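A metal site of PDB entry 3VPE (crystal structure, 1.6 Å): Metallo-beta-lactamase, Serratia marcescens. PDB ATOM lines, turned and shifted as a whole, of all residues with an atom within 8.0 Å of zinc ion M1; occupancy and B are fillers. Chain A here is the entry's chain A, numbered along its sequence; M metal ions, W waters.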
ATOM      1  N   TRP A   5     -16.138   9.353 -22.706  1.00  0.00           N
ATOM      2  CA  TRP A   5     -14.803   8.894 -23.046  1.00  0.00           C
ATOM      3  C   TRP A   5     -13.850   9.995 -23.374  1.00  0.00           C
ATOM      4  O   TRP A   5     -12.628   9.827 -23.232  1.00  0.00           O
ATOM      5  CB  TRP A   5     -14.879   7.929 -24.222  1.00  0.00           C
ATOM      6  CG  TRP A   5     -15.551   6.614 -23.922  1.00  0.00           C
ATOM      7  CD1 TRP A   5     -15.901   6.059 -22.695  1.00  0.00           C
ATOM      8  CD2 TRP A   5     -15.940   5.598 -24.913  1.00  0.00           C
ATOM      9  NE1 TRP A   5     -16.464   4.814 -22.850  1.00  0.00           N
ATOM     10  CE2 TRP A   5     -16.527   4.487 -24.159  1.00  0.00           C
ATOM     11  CE3 TRP A   5     -15.867   5.511 -26.302  1.00  0.00           C
ATOM     12  CZ2 TRP A   5     -16.995   3.337 -24.788  1.00  0.00           C
ATOM     13  CZ3 TRP A   5     -16.349   4.350 -26.914  1.00  0.00           C
ATOM     14  CH2 TRP A   5     -16.898   3.305 -26.178  1.00  0.00           C
ATOM     15  N   ILE A  26     -12.071   7.324 -19.614  1.00  0.00           N
ATOM     16  CA  ILE A  26     -11.040   6.361 -20.077  1.00  0.00           C
ATOM     17  C   ILE A  26      -9.726   6.634 -19.368  1.00  0.00           C
ATOM     18  O   ILE A  26      -9.230   7.779 -19.316  1.00  0.00           O
ATOM     19  CB  ILE A  26     -10.787   6.453 -21.594  1.00  0.00           C
ATOM     20  CG1 ILE A  26     -12.058   6.151 -22.403  1.00  0.00           C
ATOM     21  CG2 ILE A  26      -9.651   5.500 -22.014  1.00  0.00           C
ATOM     22  CD1 ILE A  26     -12.502   4.701 -22.321  1.00  0.00           C
ATOM     23  N   THR A  71      -2.786  -0.674 -24.089  1.00  0.00           N
ATOM     24  CA  THR A  71      -3.506  -1.876 -23.617  1.00  0.00           C
ATOM     25  C   THR A  71      -4.118  -2.609 -24.810  1.00  0.00           C
ATOM     26  O   THR A  71      -3.746  -3.744 -25.089  1.00  0.00           O
ATOM     27  CB  THR A  71      -4.620  -1.533 -22.603  1.00  0.00           C
ATOM     28  OG1 THR A  71      -5.466  -0.506 -23.145  1.00  0.00           O
ATOM     29  CG2 THR A  71      -3.999  -1.087 -21.247  1.00  0.00           C
ATOM     30  N   HIS A  72      -5.055  -1.973 -25.510  1.00  0.00           N
ATOM     31  CA  HIS A  72      -5.589  -2.611 -26.703  1.00  0.00           C
ATOM     32  C   HIS A  72      -6.056  -1.580 -27.704  1.00  0.00           C
ATOM     33  O   HIS A  72      -6.302  -0.403 -27.379  1.00  0.00           O
ATOM     34  CB  HIS A  72      -6.680  -3.647 -26.356  1.00  0.00           C
ATOM     35  CG  HIS A  72      -7.969  -3.049 -25.872  1.00  0.00           C
ATOM     36  ND1 HIS A  72      -8.250  -2.856 -24.580  1.00  0.00           N
ATOM     37  CD2 HIS A  72      -9.113  -2.648 -26.575  1.00  0.00           C
ATOM     38  CE1 HIS A  72      -9.491  -2.338 -24.434  1.00  0.00           C
ATOM     39  NE2 HIS A  72     -10.013  -2.203 -25.667  1.00  0.00           N
ATOM     40  N   SER A  73      -6.171  -2.051 -28.947  1.00  0.00           N
ATOM     41  CA  SER A  73      -6.362  -1.201 -30.128  1.00  0.00           C
ATOM     42  C   SER A  73      -7.839  -0.923 -30.477  1.00  0.00           C
ATOM     43  O   SER A  73      -8.290  -1.216 -31.616  1.00  0.00           O
ATOM     44  CB  SER A  73      -5.563  -1.821 -31.288  1.00  0.00           C
ATOM     45  OG  SER A  73      -5.912  -3.189 -31.422  1.00  0.00           O
ATOM     46  N   HIS A  74      -8.606  -0.417 -29.504  1.00  0.00           N
ATOM     47  CA  HIS A  74      -9.954   0.104 -29.759  1.00  0.00           C
ATOM     48  C   HIS A  74      -9.894   1.597 -29.660  1.00  0.00           C
ATOM     49  O   HIS A  74      -9.082   2.114 -28.871  1.00  0.00           O
ATOM     50  CB  HIS A  74     -10.955  -0.450 -28.773  1.00  0.00           C
ATOM     51  CG  HIS A  74     -11.339  -1.871 -29.047  1.00  0.00           C
ATOM     52  ND1 HIS A  74     -11.890  -2.661 -28.108  1.00  0.00           N
ATOM     53  CD2 HIS A  74     -11.262  -2.627 -30.206  1.00  0.00           C
ATOM     54  CE1 HIS A  74     -12.141  -3.862 -28.655  1.00  0.00           C
ATOM     55  NE2 HIS A  74     -11.751  -3.840 -29.940  1.00  0.00           N
ATOM     56  N   GLU A  75     -10.757   2.279 -30.412  1.00  0.00           N
ATOM     57  CA  GLU A  75     -10.727   3.728 -30.474  1.00  0.00           C
ATOM     58  C   GLU A  75     -10.809   4.436 -29.123  1.00  0.00           C
ATOM     59  O   GLU A  75     -10.249   5.534 -28.988  1.00  0.00           O
ATOM     60  CB  GLU A  75     -11.831   4.287 -31.415  1.00  0.00           C
ATOM     61  CG  GLU A  75     -13.259   4.016 -30.964  1.00  0.00           C
ATOM     62  CD  GLU A  75     -13.897   5.183 -30.200  1.00  0.00           C
ATOM     63  OE1 GLU A  75     -13.232   6.227 -29.990  1.00  0.00           O
ATOM     64  OE2 GLU A  75     -15.084   5.057 -29.826  1.00  0.00           O
ATOM     65  N   ASP A  76     -11.507   3.841 -28.158  1.00  0.00           N
ATOM     66  CA  ASP A  76     -11.701   4.504 -26.855  1.00  0.00           C
ATOM     67  C   ASP A  76     -10.401   4.569 -26.030  1.00  0.00           C
ATOM     68  O   ASP A  76     -10.264   5.468 -25.180  1.00  0.00           O
ATOM     69  CB  ASP A  76     -12.907   3.961 -26.049  1.00  0.00           C
ATOM     70  CG  ASP A  76     -12.882   2.460 -25.824  1.00  0.00           C
ATOM     71  OD1 ASP A  76     -12.421   1.710 -26.724  1.00  0.00           O
ATOM     72  OD2 ASP A  76     -13.398   2.030 -24.759  1.00  0.00           O
ATOM     73  N   HIS A  77      -9.467   3.649 -26.307  1.00  0.00           N
ATOM     74  CA  HIS A  77      -8.144   3.639 -25.601  1.00  0.00           C
ATOM     75  C   HIS A  77      -6.979   4.105 -26.430  1.00  0.00           C
ATOM     76  O   HIS A  77      -5.996   4.646 -25.899  1.00  0.00           O
ATOM     77  CB  HIS A  77      -7.840   2.224 -25.054  1.00  0.00           C
ATOM     78  CG  HIS A  77      -8.974   1.678 -24.250  1.00  0.00           C
ATOM     79  ND1 HIS A  77      -9.157   1.961 -22.919  1.00  0.00           N
ATOM     80  CD2 HIS A  77     -10.082   0.948 -24.663  1.00  0.00           C
ATOM     81  CE1 HIS A  77     -10.281   1.363 -22.497  1.00  0.00           C
ATOM     82  NE2 HIS A  77     -10.868   0.753 -23.564  1.00  0.00           N
ATOM     83  N   ASP A 111     -11.525  -8.981 -34.908  1.00  0.00           N
ATOM     84  CA  ASP A 111     -11.772  -8.287 -33.646  1.00  0.00           C
ATOM     85  C   ASP A 111     -13.253  -8.318 -33.266  1.00  0.00           C
ATOM     86  O   ASP A 111     -14.111  -8.047 -34.110  1.00  0.00           O
ATOM     87  CB  ASP A 111     -11.287  -6.853 -33.728  1.00  0.00           C
ATOM     88  CG  ASP A 111     -11.184  -6.206 -32.377  1.00  0.00           C
ATOM     89  OD1 ASP A 111     -10.064  -6.180 -31.825  1.00  0.00           O
ATOM     90  OD2 ASP A 111     -12.227  -5.764 -31.862  1.00  0.00           O
ATOM     91  N   GLN A 113     -15.024  -6.240 -31.809  1.00  0.00           N
ATOM     92  CA  GLN A 113     -15.656  -4.932 -32.030  1.00  0.00           C
ATOM     93  C   GLN A 113     -15.243  -4.338 -33.359  1.00  0.00           C
ATOM     94  O   GLN A 113     -15.295  -3.110 -33.563  1.00  0.00           O
ATOM     95  CB  GLN A 113     -15.419  -3.968 -30.852  1.00  0.00           C
ATOM     96  CG  GLN A 113     -16.172  -4.444 -29.625  1.00  0.00           C
ATOM     97  CD  GLN A 113     -16.216  -3.458 -28.488  1.00  0.00           C
ATOM     98  OE1 GLN A 113     -16.967  -2.514 -28.526  1.00  0.00           O
ATOM     99  NE2 GLN A 113     -15.397  -3.692 -27.451  1.00  0.00           N
ATOM    100  N   LEU A 117     -17.134  -0.491 -33.370  1.00  0.00           N
ATOM    101  CA  LEU A 117     -16.285   0.648 -32.974  1.00  0.00           C
ATOM    102  C   LEU A 117     -15.620   1.220 -34.220  1.00  0.00           C
ATOM    103  O   LEU A 117     -15.345   0.497 -35.168  1.00  0.00           O
ATOM    104  CB  LEU A 117     -15.240   0.211 -31.925  1.00  0.00           C
ATOM    105  CG  LEU A 117     -15.808  -0.043 -30.523  1.00  0.00           C
ATOM    106  CD1 LEU A 117     -14.685  -0.327 -29.529  1.00  0.00           C
ATOM    107  CD2 LEU A 117     -16.609   1.132 -29.982  1.00  0.00           C
ATOM    108  N   HIS A 150     -10.551  -9.749 -25.343  1.00  0.00           N
ATOM    109  CA  HIS A 150     -11.291  -8.557 -25.800  1.00  0.00           C
ATOM    110  C   HIS A 150     -10.732  -8.045 -27.123  1.00  0.00           C
ATOM    111  O   HIS A 150     -11.501  -7.507 -27.963  1.00  0.00           O
ATOM    112  CB  HIS A 150     -11.216  -7.540 -24.643  1.00  0.00           C
ATOM    113  CG  HIS A 150     -11.897  -6.229 -24.891  1.00  0.00           C
ATOM    114  ND1 HIS A 150     -13.177  -5.967 -24.522  1.00  0.00           N
ATOM    115  CD2 HIS A 150     -11.387  -5.056 -25.411  1.00  0.00           C
ATOM    116  CE1 HIS A 150     -13.463  -4.681 -24.829  1.00  0.00           C
ATOM    117  NE2 HIS A 150     -12.388  -4.132 -25.389  1.00  0.00           N
ATOM    118  N   THR A 151      -9.405  -8.163 -27.302  1.00  0.00           N
ATOM    119  CA  THR A 151      -8.691  -8.059 -28.582  1.00  0.00           C
ATOM    120  C   THR A 151      -7.588  -9.118 -28.582  1.00  0.00           C
ATOM    121  O   THR A 151      -7.215  -9.612 -27.506  1.00  0.00           O
ATOM    122  CB  THR A 151      -8.010  -6.707 -28.829  1.00  0.00           C
ATOM    123  OG1 THR A 151      -6.916  -6.553 -27.903  1.00  0.00           O
ATOM    124  CG2 THR A 151      -9.006  -5.563 -28.696  1.00  0.00           C
ATOM    125  N   ASP A 174      -5.795  -4.274 -18.637  1.00  0.00           N
ATOM    126  CA  ASP A 174      -6.523  -4.232 -19.898  1.00  0.00           C
ATOM    127  C   ASP A 174      -7.940  -4.746 -19.653  1.00  0.00           C
ATOM    128  O   ASP A 174      -8.242  -5.434 -18.661  1.00  0.00           O
ATOM    129  CB  ASP A 174      -5.808  -5.122 -20.907  1.00  0.00           C
ATOM    130  CG  ASP A 174      -6.335  -4.955 -22.322  1.00  0.00           C
ATOM    131  OD1 ASP A 174      -6.939  -3.874 -22.588  1.00  0.00           O
ATOM    132  OD2 ASP A 174      -6.087  -5.869 -23.136  1.00  0.00           O
ATOM    133  N   SER A 175      -8.816  -4.436 -20.600  1.00  0.00           N
ATOM    134  CA  SER A 175     -10.217  -4.916 -20.506  1.00  0.00           C
ATOM    135  C   SER A 175     -10.347  -6.390 -20.730  1.00  0.00           C
ATOM    136  O   SER A 175      -9.738  -6.922 -21.661  1.00  0.00           O
ATOM    137  CB  SER A 175     -11.026  -4.213 -21.593  1.00  0.00           C
ATOM    138  OG  SER A 175     -10.973  -2.814 -21.391  1.00  0.00           O
ATOM    139  N   LEU A 176     -11.152  -7.040 -19.896  1.00  0.00           N
ATOM    140  CA  LEU A 176     -11.342  -8.488 -19.950  1.00  0.00           C
ATOM    141  C   LEU A 176     -12.795  -8.812 -20.284  1.00  0.00           C
ATOM    142  O   LEU A 176     -13.292  -9.895 -19.958  1.00  0.00           O
ATOM    143  CB  LEU A 176     -10.969  -9.140 -18.620  1.00  0.00           C
ATOM    144  CG  LEU A 176      -9.542  -8.845 -18.116  1.00  0.00           C
ATOM    145  CD1 LEU A 176      -9.226  -9.610 -16.817  1.00  0.00           C
ATOM    146  CD2 LEU A 176      -8.464  -9.136 -19.177  1.00  0.00           C
ATOM    147  N   THR A 177     -13.444  -7.856 -20.952  1.00  0.00           N
ATOM    148  CA  THR A 177     -14.895  -7.963 -21.222  1.00  0.00           C
ATOM    149  C   THR A 177     -15.263  -8.610 -22.578  1.00  0.00           C
ATOM    150  O   THR A 177     -14.732  -8.219 -23.641  1.00  0.00           O
ATOM    151  CB  THR A 177     -15.504  -6.570 -21.198  1.00  0.00           C
ATOM    152  OG1 THR A 177     -14.721  -5.694 -22.030  1.00  0.00           O
ATOM    153  CG2 THR A 177     -15.510  -6.047 -19.747  1.00  0.00           C
ATOM    154  N   VAL A 179     -17.403  -8.244 -24.897  1.00  0.00           N
ATOM    155  CA  VAL A 179     -18.317  -7.336 -25.605  1.00  0.00           C
ATOM    156  C   VAL A 179     -17.949  -7.289 -27.080  1.00  0.00           C
ATOM    157  O   VAL A 179     -16.807  -7.586 -27.445  1.00  0.00           O
ATOM    158  CB  VAL A 179     -18.311  -5.948 -24.957  1.00  0.00           C
ATOM    159  CG1 VAL A 179     -18.951  -6.025 -23.577  1.00  0.00           C
ATOM    160  CG2 VAL A 179     -16.882  -5.415 -24.868  1.00  0.00           C
ATOM    161  N   ALA A 214      -8.630  -0.092 -17.455  1.00  0.00           N
ATOM    162  CA  ALA A 214      -8.697   0.733 -18.658  1.00  0.00           C
ATOM    163  C   ALA A 214      -9.979   1.594 -18.706  1.00  0.00           C
ATOM    164  O   ALA A 214      -9.890   2.751 -19.066  1.00  0.00           O
ATOM    165  CB  ALA A 214      -8.535  -0.156 -19.893  1.00  0.00           C
ATOM    166  N   HIS A 215     -11.123   1.001 -18.322  1.00  0.00           N
ATOM    167  CA  HIS A 215     -12.304   1.782 -17.964  1.00  0.00           C
ATOM    168  C   HIS A 215     -12.237   1.957 -16.467  1.00  0.00           C
ATOM    169  O   HIS A 215     -12.420   0.986 -15.733  1.00  0.00           O
ATOM    170  CB  HIS A 215     -13.558   1.042 -18.405  1.00  0.00           C
ATOM    171  CG  HIS A 215     -13.757   1.075 -19.892  1.00  0.00           C
ATOM    172  ND1 HIS A 215     -14.464   2.058 -20.504  1.00  0.00           N
ATOM    173  CD2 HIS A 215     -13.305   0.218 -20.887  1.00  0.00           C
ATOM    174  CE1 HIS A 215     -14.423   1.880 -21.844  1.00  0.00           C
ATOM    175  NE2 HIS A 215     -13.725   0.739 -22.094  1.00  0.00           N
HETATM  176 ZN    ZN M   1     -12.024  -2.300 -26.097  1.00  0.00          ZN
HETATM  177 ZN    ZN M   2     -12.827   0.207 -23.864  1.00  0.00          ZN
HETATM  178  O   HOH W   1     -13.141  -0.729 -25.672  1.00  0.00           O
HETATM  179  O   HOH W   2     -12.695  -1.878 -23.133  1.00  0.00           O
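ND1 of His 150 lies within hydrogen-bond range of O of Thr 177, 2.9 Å away. OD1 of Asp 174 lies within hydrogen-bond range of ND1 of His 72 (2.6 Å). The backbone NH (N) of Gln 113 lies within hydrogen-bond range of the side-chain carboxylate (OD2) of Asp 111. OD2 of Asp 111 is in hydrogen-bond range of NE2 of His 74 (2.8 Å).
Water W1 is bound to zinc ion M1 (2.0 Å). A ring nitrogen (NE2) of His 150 binds zinc ion M1 (2.0 Å). Zinc ion M1 is bound by ND1 of His 74, at 2.0 Å. NE2 of His 72 is bound to zinc ion M1 (2.1 Å).
Residues that only touch zinc ion M1: Gln 113 (3.9 Å). The nearest printed residue that does not touch zinc ion M1 is His 77 (4.05 Å).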
